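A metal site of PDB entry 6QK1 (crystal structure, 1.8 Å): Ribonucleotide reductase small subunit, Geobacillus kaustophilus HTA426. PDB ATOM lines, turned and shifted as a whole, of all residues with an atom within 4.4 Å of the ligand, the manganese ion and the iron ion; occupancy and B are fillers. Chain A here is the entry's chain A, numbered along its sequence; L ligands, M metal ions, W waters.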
ATOM      1  N   LEU A  75      -8.440 -13.640 -20.839  1.00  0.00           N
ATOM      2  CA  LEU A  75      -7.382 -13.096 -19.984  1.00  0.00           C
ATOM      3  C   LEU A  75      -6.325 -14.145 -19.703  1.00  0.00           C
ATOM      4  O   LEU A  75      -5.129 -13.835 -19.713  1.00  0.00           O
ATOM      5  CB  LEU A  75      -7.999 -12.573 -18.677  1.00  0.00           C
ATOM      6  CG  LEU A  75      -7.111 -11.820 -17.703  1.00  0.00           C
ATOM      7  CD1 LEU A  75      -6.485 -10.599 -18.387  1.00  0.00           C
ATOM      8  CD2 LEU A  75      -7.912 -11.386 -16.428  1.00  0.00           C
ATOM      9  N   GLY A  78      -4.178 -14.495 -22.729  1.00  0.00           N
ATOM     10  CA  GLY A  78      -3.175 -13.443 -22.807  1.00  0.00           C
ATOM     11  C   GLY A  78      -2.003 -13.652 -21.861  1.00  0.00           C
ATOM     12  O   GLY A  78      -0.851 -13.388 -22.214  1.00  0.00           O
ATOM     13  N   PHE A  79      -2.280 -14.106 -20.631  1.00  0.00           N
ATOM     14  CA  PHE A  79      -1.212 -14.339 -19.674  1.00  0.00           C
ATOM     15  C   PHE A  79      -0.355 -15.553 -20.047  1.00  0.00           C
ATOM     16  O   PHE A  79       0.873 -15.481 -19.961  1.00  0.00           O
ATOM     17  CB  PHE A  79      -1.771 -14.497 -18.268  1.00  0.00           C
ATOM     18  CG  PHE A  79      -1.730 -13.223 -17.473  1.00  0.00           C
ATOM     19  CD1 PHE A  79      -0.537 -12.799 -16.914  1.00  0.00           C
ATOM     20  CD2 PHE A  79      -2.860 -12.437 -17.310  1.00  0.00           C
ATOM     21  CE1 PHE A  79      -0.468 -11.599 -16.170  1.00  0.00           C
ATOM     22  CE2 PHE A  79      -2.804 -11.268 -16.556  1.00  0.00           C
ATOM     23  CZ  PHE A  79      -1.605 -10.840 -16.015  1.00  0.00           C
ATOM     24  N   GLY A  82       1.891 -14.662 -22.690  1.00  0.00           N
ATOM     25  CA  GLY A  82       2.788 -13.607 -22.272  1.00  0.00           C
ATOM     26  C   GLY A  82       3.915 -14.113 -21.412  1.00  0.00           C
ATOM     27  O   GLY A  82       5.081 -13.755 -21.618  1.00  0.00           O
ATOM     28  N   GLU A  83       3.595 -14.981 -20.427  1.00  0.00           N
ATOM     29  CA  GLU A  83       4.606 -15.574 -19.564  1.00  0.00           C
ATOM     30  C   GLU A  83       5.570 -16.427 -20.379  1.00  0.00           C
ATOM     31  O   GLU A  83       6.771 -16.468 -20.112  1.00  0.00           O
ATOM     32  CB  GLU A  83       4.005 -16.431 -18.469  1.00  0.00           C
ATOM     33  CG  GLU A  83       2.940 -15.785 -17.598  1.00  0.00           C
ATOM     34  CD  GLU A  83       3.442 -14.623 -16.763  1.00  0.00           C
ATOM     35  OE1 GLU A  83       2.591 -13.869 -16.224  1.00  0.00           O
ATOM     36  OE2 GLU A  83       4.684 -14.475 -16.665  1.00  0.00           O
ATOM     37  N   VAL A  86       7.964 -14.102 -22.422  1.00  0.00           N
ATOM     38  CA  VAL A  86       9.022 -13.430 -21.657  1.00  0.00           C
ATOM     39  C   VAL A  86      10.029 -14.448 -21.103  1.00  0.00           C
ATOM     40  O   VAL A  86      11.226 -14.142 -20.984  1.00  0.00           O
ATOM     41  CB  VAL A  86       8.404 -12.545 -20.547  1.00  0.00           C
ATOM     42  CG1 VAL A  86       7.603 -11.433 -21.146  1.00  0.00           C
ATOM     43  CG2 VAL A  86       7.651 -13.336 -19.491  1.00  0.00           C
ATOM     44  N   PHE A 112      15.048 -13.579 -12.250  1.00  0.00           N
ATOM     45  CA  PHE A 112      14.033 -13.067 -13.144  1.00  0.00           C
ATOM     46  C   PHE A 112      13.535 -14.190 -14.056  1.00  0.00           C
ATOM     47  O   PHE A 112      12.311 -14.430 -14.191  1.00  0.00           O
ATOM     48  CB  PHE A 112      14.661 -11.909 -13.940  1.00  0.00           C
ATOM     49  CG  PHE A 112      13.725 -11.059 -14.759  1.00  0.00           C
ATOM     50  CD1 PHE A 112      13.834  -9.684 -14.699  1.00  0.00           C
ATOM     51  CD2 PHE A 112      12.864 -11.581 -15.690  1.00  0.00           C
ATOM     52  CE1 PHE A 112      13.056  -8.862 -15.457  1.00  0.00           C
ATOM     53  CE2 PHE A 112      12.069 -10.768 -16.478  1.00  0.00           C
ATOM     54  CZ  PHE A 112      12.160  -9.393 -16.381  1.00  0.00           C
ATOM     55  N   GLU A 116       9.841 -16.281 -14.250  1.00  0.00           N
ATOM     56  CA  GLU A 116       8.958 -16.395 -15.408  1.00  0.00           C
ATOM     57  C   GLU A 116       8.611 -17.848 -15.680  1.00  0.00           C
ATOM     58  O   GLU A 116       7.489 -18.158 -16.078  1.00  0.00           O
ATOM     59  CB  GLU A 116       9.583 -15.748 -16.653  1.00  0.00           C
ATOM     60  CG  GLU A 116       9.945 -14.236 -16.503  1.00  0.00           C
ATOM     61  CD  GLU A 116       8.724 -13.346 -16.217  1.00  0.00           C
ATOM     62  OE1 GLU A 116       8.899 -12.129 -16.170  1.00  0.00           O
ATOM     63  OE2 GLU A 116       7.572 -13.818 -16.119  1.00  0.00           O
ATOM     64  N   HIS A 119       5.904 -18.712 -13.566  1.00  0.00           N
ATOM     65  CA  HIS A 119       4.655 -18.084 -14.005  1.00  0.00           C
ATOM     66  C   HIS A 119       4.006 -18.881 -15.143  1.00  0.00           C
ATOM     67  O   HIS A 119       2.772 -19.063 -15.170  1.00  0.00           O
ATOM     68  CB  HIS A 119       4.869 -16.666 -14.463  1.00  0.00           C
ATOM     69  CG  HIS A 119       5.418 -15.772 -13.402  1.00  0.00           C
ATOM     70  ND1 HIS A 119       5.750 -14.446 -13.622  1.00  0.00           N
ATOM     71  CD2 HIS A 119       5.724 -16.041 -12.106  1.00  0.00           C
ATOM     72  CE1 HIS A 119       6.207 -13.938 -12.479  1.00  0.00           C
ATOM     73  NE2 HIS A 119       6.235 -14.885 -11.562  1.00  0.00           N
ATOM     74  N   PHE A 149       3.380  -9.346 -28.677  1.00  0.00           N
ATOM     75  CA  PHE A 149       3.981 -10.535 -28.091  1.00  0.00           C
ATOM     76  C   PHE A 149       4.590 -11.485 -29.111  1.00  0.00           C
ATOM     77  O   PHE A 149       5.587 -12.156 -28.794  1.00  0.00           O
ATOM     78  CB  PHE A 149       2.953 -11.275 -27.263  1.00  0.00           C
ATOM     79  CG  PHE A 149       2.653 -10.611 -25.951  1.00  0.00           C
ATOM     80  CD1 PHE A 149       3.474 -10.815 -24.847  1.00  0.00           C
ATOM     81  CD2 PHE A 149       1.567  -9.754 -25.831  1.00  0.00           C
ATOM     82  CE1 PHE A 149       3.193 -10.182 -23.644  1.00  0.00           C
ATOM     83  CE2 PHE A 149       1.287  -9.142 -24.633  1.00  0.00           C
ATOM     84  CZ  PHE A 149       2.108  -9.358 -23.542  1.00  0.00           C
ATOM     85  N   VAL A 180       5.198  -4.551 -21.442  1.00  0.00           N
ATOM     86  CA  VAL A 180       4.621  -5.888 -21.214  1.00  0.00           C
ATOM     87  C   VAL A 180       4.372  -6.129 -19.717  1.00  0.00           C
ATOM     88  O   VAL A 180       3.271  -6.562 -19.310  1.00  0.00           O
ATOM     89  CB  VAL A 180       5.535  -6.958 -21.837  1.00  0.00           C
ATOM     90  CG1 VAL A 180       5.247  -8.341 -21.288  1.00  0.00           C
ATOM     91  CG2 VAL A 180       5.408  -6.890 -23.357  1.00  0.00           C
ATOM     92  N   GLU A 181       5.381  -5.876 -18.872  1.00  0.00           N
ATOM     93  CA  GLU A 181       5.285  -6.122 -17.431  1.00  0.00           C
ATOM     94  C   GLU A 181       4.636  -4.940 -16.741  1.00  0.00           C
ATOM     95  O   GLU A 181       3.644  -5.085 -16.009  1.00  0.00           O
ATOM     96  CB  GLU A 181       6.667  -6.408 -16.809  1.00  0.00           C
ATOM     97  CG  GLU A 181       7.383  -7.649 -17.370  1.00  0.00           C
ATOM     98  CD  GLU A 181       8.726  -7.899 -16.732  1.00  0.00           C
ATOM     99  OE1 GLU A 181       9.496  -6.930 -16.543  1.00  0.00           O
ATOM    100  OE2 GLU A 181       9.002  -9.054 -16.352  1.00  0.00           O
ATOM    101  N   LEU A 184       0.934  -3.920 -19.094  1.00  0.00           N
ATOM    102  CA  LEU A 184      -0.076  -4.940 -19.370  1.00  0.00           C
ATOM    103  C   LEU A 184      -0.202  -5.913 -18.210  1.00  0.00           C
ATOM    104  O   LEU A 184      -1.325  -6.177 -17.738  1.00  0.00           O
ATOM    105  CB  LEU A 184       0.252  -5.680 -20.679  1.00  0.00           C
ATOM    106  CG  LEU A 184      -0.034  -4.920 -21.951  1.00  0.00           C
ATOM    107  CD1 LEU A 184       0.611  -5.626 -23.161  1.00  0.00           C
ATOM    108  CD2 LEU A 184      -1.520  -4.717 -22.216  1.00  0.00           C
ATOM    109  N   ALA A 185       0.920  -6.486 -17.749  1.00  0.00           N
ATOM    110  CA  ALA A 185       0.846  -7.451 -16.655  1.00  0.00           C
ATOM    111  C   ALA A 185       0.188  -6.845 -15.408  1.00  0.00           C
ATOM    112  O   ALA A 185      -0.696  -7.452 -14.769  1.00  0.00           O
ATOM    113  CB  ALA A 185       2.236  -7.974 -16.293  1.00  0.00           C
ATOM    114  N   SER A 187      -1.832  -4.409 -15.085  1.00  0.00           N
ATOM    115  CA  SER A 187      -3.247  -4.179 -15.296  1.00  0.00           C
ATOM    116  C   SER A 187      -4.015  -5.498 -15.306  1.00  0.00           C
ATOM    117  O   SER A 187      -5.149  -5.551 -14.843  1.00  0.00           O
ATOM    118  CB  SER A 187      -3.507  -3.415 -16.601  1.00  0.00           C
ATOM    119  OG  SER A 187      -2.852  -2.168 -16.659  1.00  0.00           O
ATOM    120  N   GLY A 188      -3.417  -6.577 -15.827  1.00  0.00           N
ATOM    121  CA  GLY A 188      -4.093  -7.870 -15.776  1.00  0.00           C
ATOM    122  C   GLY A 188      -4.195  -8.416 -14.375  1.00  0.00           C
ATOM    123  O   GLY A 188      -5.190  -9.062 -14.024  1.00  0.00           O
ATOM    124  N   THR A 191      -7.085  -6.537 -13.015  1.00  0.00           N
ATOM    125  CA  THR A 191      -8.339  -7.028 -13.601  1.00  0.00           C
ATOM    126  C   THR A 191      -8.773  -8.347 -12.948  1.00  0.00           C
ATOM    127  O   THR A 191      -9.961  -8.527 -12.642  1.00  0.00           O
ATOM    128  CB  THR A 191      -8.160  -7.168 -15.115  1.00  0.00           C
ATOM    129  OG1 THR A 191      -7.838  -5.903 -15.679  1.00  0.00           O
ATOM    130  CG2 THR A 191      -9.388  -7.709 -15.801  1.00  0.00           C
ATOM    131  N   GLU A 216       6.758  -9.686 -10.024  1.00  0.00           N
ATOM    132  CA  GLU A 216       6.757  -8.684 -11.082  1.00  0.00           C
ATOM    133  C   GLU A 216       7.331  -7.365 -10.597  1.00  0.00           C
ATOM    134  O   GLU A 216       7.967  -6.639 -11.363  1.00  0.00           O
ATOM    135  CB  GLU A 216       5.340  -8.446 -11.554  1.00  0.00           C
ATOM    136  CG  GLU A 216       5.273  -7.894 -12.894  1.00  0.00           C
ATOM    137  CD  GLU A 216       5.607  -8.999 -13.863  1.00  0.00           C
ATOM    138  OE1 GLU A 216       4.780  -9.923 -13.985  1.00  0.00           O
ATOM    139  OE2 GLU A 216       6.730  -8.972 -14.402  1.00  0.00           O
ATOM    140  N   HIS A 219      10.947  -7.377 -11.322  1.00  0.00           N
ATOM    141  CA  HIS A 219      11.199  -7.262 -12.760  1.00  0.00           C
ATOM    142  C   HIS A 219      11.104  -5.808 -13.233  1.00  0.00           C
ATOM    143  O   HIS A 219      11.951  -5.332 -13.982  1.00  0.00           O
ATOM    144  CB  HIS A 219      10.209  -8.148 -13.530  1.00  0.00           C
ATOM    145  CG  HIS A 219      10.209  -9.573 -13.095  1.00  0.00           C
ATOM    146  ND1 HIS A 219       9.428 -10.545 -13.692  1.00  0.00           N
ATOM    147  CD2 HIS A 219      10.895 -10.203 -12.107  1.00  0.00           C
ATOM    148  CE1 HIS A 219       9.621 -11.698 -13.069  1.00  0.00           C
ATOM    149  NE2 HIS A 219      10.517 -11.512 -12.117  1.00  0.00           N
ATOM    150  N   TYR A 255      -5.456  -3.912 -27.696  1.00  0.00           N
ATOM    151  CA  TYR A 255      -5.728  -5.186 -27.072  1.00  0.00           C
ATOM    152  C   TYR A 255      -6.714  -5.023 -25.906  1.00  0.00           C
ATOM    153  O   TYR A 255      -7.618  -5.853 -25.718  1.00  0.00           O
ATOM    154  CB  TYR A 255      -4.425  -5.819 -26.615  1.00  0.00           C
ATOM    155  CG  TYR A 255      -4.595  -7.110 -25.850  1.00  0.00           C
ATOM    156  CD1 TYR A 255      -5.268  -8.207 -26.405  1.00  0.00           C
ATOM    157  CD2 TYR A 255      -4.083  -7.253 -24.559  1.00  0.00           C
ATOM    158  CE1 TYR A 255      -5.409  -9.400 -25.682  1.00  0.00           C
ATOM    159  CE2 TYR A 255      -4.224  -8.446 -23.836  1.00  0.00           C
ATOM    160  CZ  TYR A 255      -4.875  -9.519 -24.410  1.00  0.00           C
ATOM    161  OH  TYR A 255      -4.999 -10.682 -23.631  1.00  0.00           O
ATOM    162  N   VAL A 256      -6.541  -3.973 -25.106  1.00  0.00           N
ATOM    163  CA  VAL A 256      -7.465  -3.693 -24.020  1.00  0.00           C
ATOM    164  C   VAL A 256      -8.880  -3.531 -24.564  1.00  0.00           C
ATOM    165  O   VAL A 256      -9.841  -4.086 -24.005  1.00  0.00           O
ATOM    166  CB  VAL A 256      -7.015  -2.443 -23.226  1.00  0.00           C
ATOM    167  CG1 VAL A 256      -8.086  -2.046 -22.220  1.00  0.00           C
ATOM    168  CG2 VAL A 256      -5.698  -2.711 -22.515  1.00  0.00           C
ATOM    169  N   LEU A 259     -10.353  -6.979 -25.548  1.00  0.00           N
ATOM    170  CA  LEU A 259     -10.797  -7.729 -24.361  1.00  0.00           C
ATOM    171  C   LEU A 259     -12.044  -7.118 -23.737  1.00  0.00           C
ATOM    172  O   LEU A 259     -12.902  -7.843 -23.225  1.00  0.00           O
ATOM    173  CB  LEU A 259      -9.698  -7.776 -23.316  1.00  0.00           C
ATOM    174  CG  LEU A 259      -8.477  -8.621 -23.602  1.00  0.00           C
ATOM    175  CD1 LEU A 259      -7.540  -8.351 -22.420  1.00  0.00           C
ATOM    176  CD2 LEU A 259      -8.829 -10.104 -23.752  1.00  0.00           C
ATOM    177  N   THR A 260     -12.124  -5.789 -23.722  1.00  0.00           N
ATOM    178  CA  THR A 260     -13.317  -5.097 -23.223  1.00  0.00           C
ATOM    179  C   THR A 260     -14.552  -5.466 -24.034  1.00  0.00           C
ATOM    180  O   THR A 260     -15.601  -5.807 -23.478  1.00  0.00           O
ATOM    181  CB  THR A 260     -13.072  -3.599 -23.248  1.00  0.00           C
ATOM    182  OG1 THR A 260     -12.143  -3.260 -22.205  1.00  0.00           O
ATOM    183  CG2 THR A 260     -14.365  -2.813 -23.056  1.00  0.00           C
ATOM    184  N   LEU A 282     -11.263  -0.267 -15.568  1.00  0.00           N
ATOM    185  CA  LEU A 282     -10.147  -1.083 -16.026  1.00  0.00           C
ATOM    186  C   LEU A 282      -9.339  -0.353 -17.077  1.00  0.00           C
ATOM    187  O   LEU A 282      -8.103  -0.287 -17.001  1.00  0.00           O
ATOM    188  CB  LEU A 282     -10.663  -2.413 -16.569  1.00  0.00           C
ATOM    189  CG  LEU A 282     -11.331  -3.405 -15.618  1.00  0.00           C
ATOM    190  CD1 LEU A 282     -11.668  -4.720 -16.343  1.00  0.00           C
ATOM    191  CD2 LEU A 282     -10.495  -3.664 -14.357  1.00  0.00           C
ATOM    192  N   VAL A 286      -5.262   1.035 -16.892  1.00  0.00           N
ATOM    193  CA  VAL A 286      -4.232   0.800 -17.918  1.00  0.00           C
ATOM    194  C   VAL A 286      -3.571   2.108 -18.286  1.00  0.00           C
ATOM    195  O   VAL A 286      -2.338   2.211 -18.321  1.00  0.00           O
ATOM    196  CB  VAL A 286      -4.851   0.137 -19.166  1.00  0.00           C
ATOM    197  CG1 VAL A 286      -3.813   0.083 -20.331  1.00  0.00           C
ATOM    198  CG2 VAL A 286      -5.326  -1.226 -18.864  1.00  0.00           C
HETATM  199  C1  LIG L   1       5.683 -11.153 -17.186  1.00  0.00           C
HETATM  200  O1  LIG L   1       6.803 -10.509 -16.850  1.00  0.00           O
HETATM  201  O2  LIG L   1       5.196 -12.167 -16.610  1.00  0.00           O
HETATM  202  C2  LIG L   1       4.817 -10.590 -18.417  1.00  0.00           C
HETATM  203  C3  LIG L   1       3.391 -11.169 -18.628  1.00  0.00           C
HETATM  204  C4  LIG L   1       2.523 -10.445 -19.626  1.00  0.00           C
HETATM  205  C5  LIG L   1       0.986 -10.698 -19.484  1.00  0.00           C
HETATM  206  C6  LIG L   1       0.209 -10.317 -20.673  1.00  0.00           C
HETATM  207  C7  LIG L   1      -1.349 -10.489 -20.552  1.00  0.00           C
HETATM  208  C8  LIG L   1      -1.959  -9.526 -19.595  1.00  0.00           C
HETATM  209  C9  LIG L   1      -3.455  -9.237 -19.833  1.00  0.00           C
HETATM  210  C10 LIG L   1      -3.739  -7.738 -20.068  1.00  0.00           C
HETATM  211  C11 LIG L   1      -5.017  -7.282 -19.438  1.00  0.00           C
HETATM  212  C12 LIG L   1      -5.214  -5.754 -19.451  1.00  0.00           C
HETATM  213  C13 LIG L   1      -6.558  -5.381 -18.798  1.00  0.00           C
HETATM  214  C14 LIG L   1      -7.720  -5.130 -19.785  1.00  0.00           C
HETATM  215  C15 LIG L   1      -9.122  -5.030 -19.141  1.00  0.00           C
HETATM  216  C16 LIG L   1     -10.181  -5.960 -19.772  1.00  0.00           C
HETATM  217 MN    MN M   1       5.677 -13.173 -15.316  1.00  0.00          MN
HETATM  218 FE    FE M   2       7.880 -10.526 -15.436  1.00  0.00          FE
HETATM  219  O   HOH W   1       3.617 -12.262 -14.596  1.00  0.00           O
HETATM  220  O   HOH W   2       6.578 -11.612 -14.015  1.00  0.00           O
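Leu 75 touches the ligand.
O of Gly 78 touches C7 of the ligand (3.4 Å).
Phe 79 touches the ligand.
Val 86 touches the ligand (CG2 to C1, 3.7 Å).
CZ of Phe 149 touches C6 of the ligand, at 3.6 Å.
Val 180 touches the ligand (CG1 to C2, 3.7 Å).
Leu 184 touches the ligand (O to C10, 3.7 Å).
CA of Gly 188 touches C11 of the ligand, at 3.8 Å.
OG1 of Thr 191 touches C13 of the ligand (3.4 Å).
CE2 of Tyr 255 touches C10 of the ligand, 3.9 Å away.
CG1 of Val 256 touches C14 of the ligand (3.9 Å).
CD1 of Leu 282 touches C15 of the ligand (3.8 Å).
Hydrophobic or aromatic side chains within 4 Å of the ligand: Leu 75, Phe 79, Val 86, Phe 149, Val 180, Tyr 255, Val 256 and Leu 282.
Of the 25 residues printed, 17 come within 4 Å of the ligand.
The nearest printed residue that does not touch the ligand is Leu 259 (4.01 Å).
O1 of the ligand binds the iron ion (1.8 Å).
OE1 of Glu 116 is bound to the iron ion (2.0 Å).
The iron ion is bound by OE2 of Glu 181, 2.1 Å away.
The side-chain carboxylate (OE2) of Glu 216 is bound to the iron ion.
The iron ion is bound by water W2, at 2.2 Å.
A ring nitrogen (ND1) of His 219 binds the iron ion.
The iron ion has six donor atoms within binding distance.
Water W1 lies within hydrogen-bond range of the side-chain carboxylate of Glu 83 and the side-chain carboxylate of Glu 216.
Within 4 Å of the manganese ion: Glu 83, Glu 116, His 119 and Glu 216.
The backbone carbonyl oxygen (O) of Val 256 lies within hydrogen-bond range of the side-chain hydroxyl (OG1) of Thr 260, 3.0 Å away.
The backbone carbonyl oxygen of Val 180 sits at hydrogen-bond distance from the backbone NH of Ala 185 (2.8 Å).
OG1 of Thr 191 sits at hydrogen-bond distance from O of Ser 187, at 2.8 Å.
The manganese ion is bound by O2 of the ligand, ND1 of His 119, OE2 of Glu 83, OE2 of Glu 116, water W2 and water W1.
Within 4 Å of the iron ion: Glu 116, Glu 181, Glu 216 and His 219.
The nearest printed residue that does not touch the iron ion is Phe 112 (4.3 Å).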
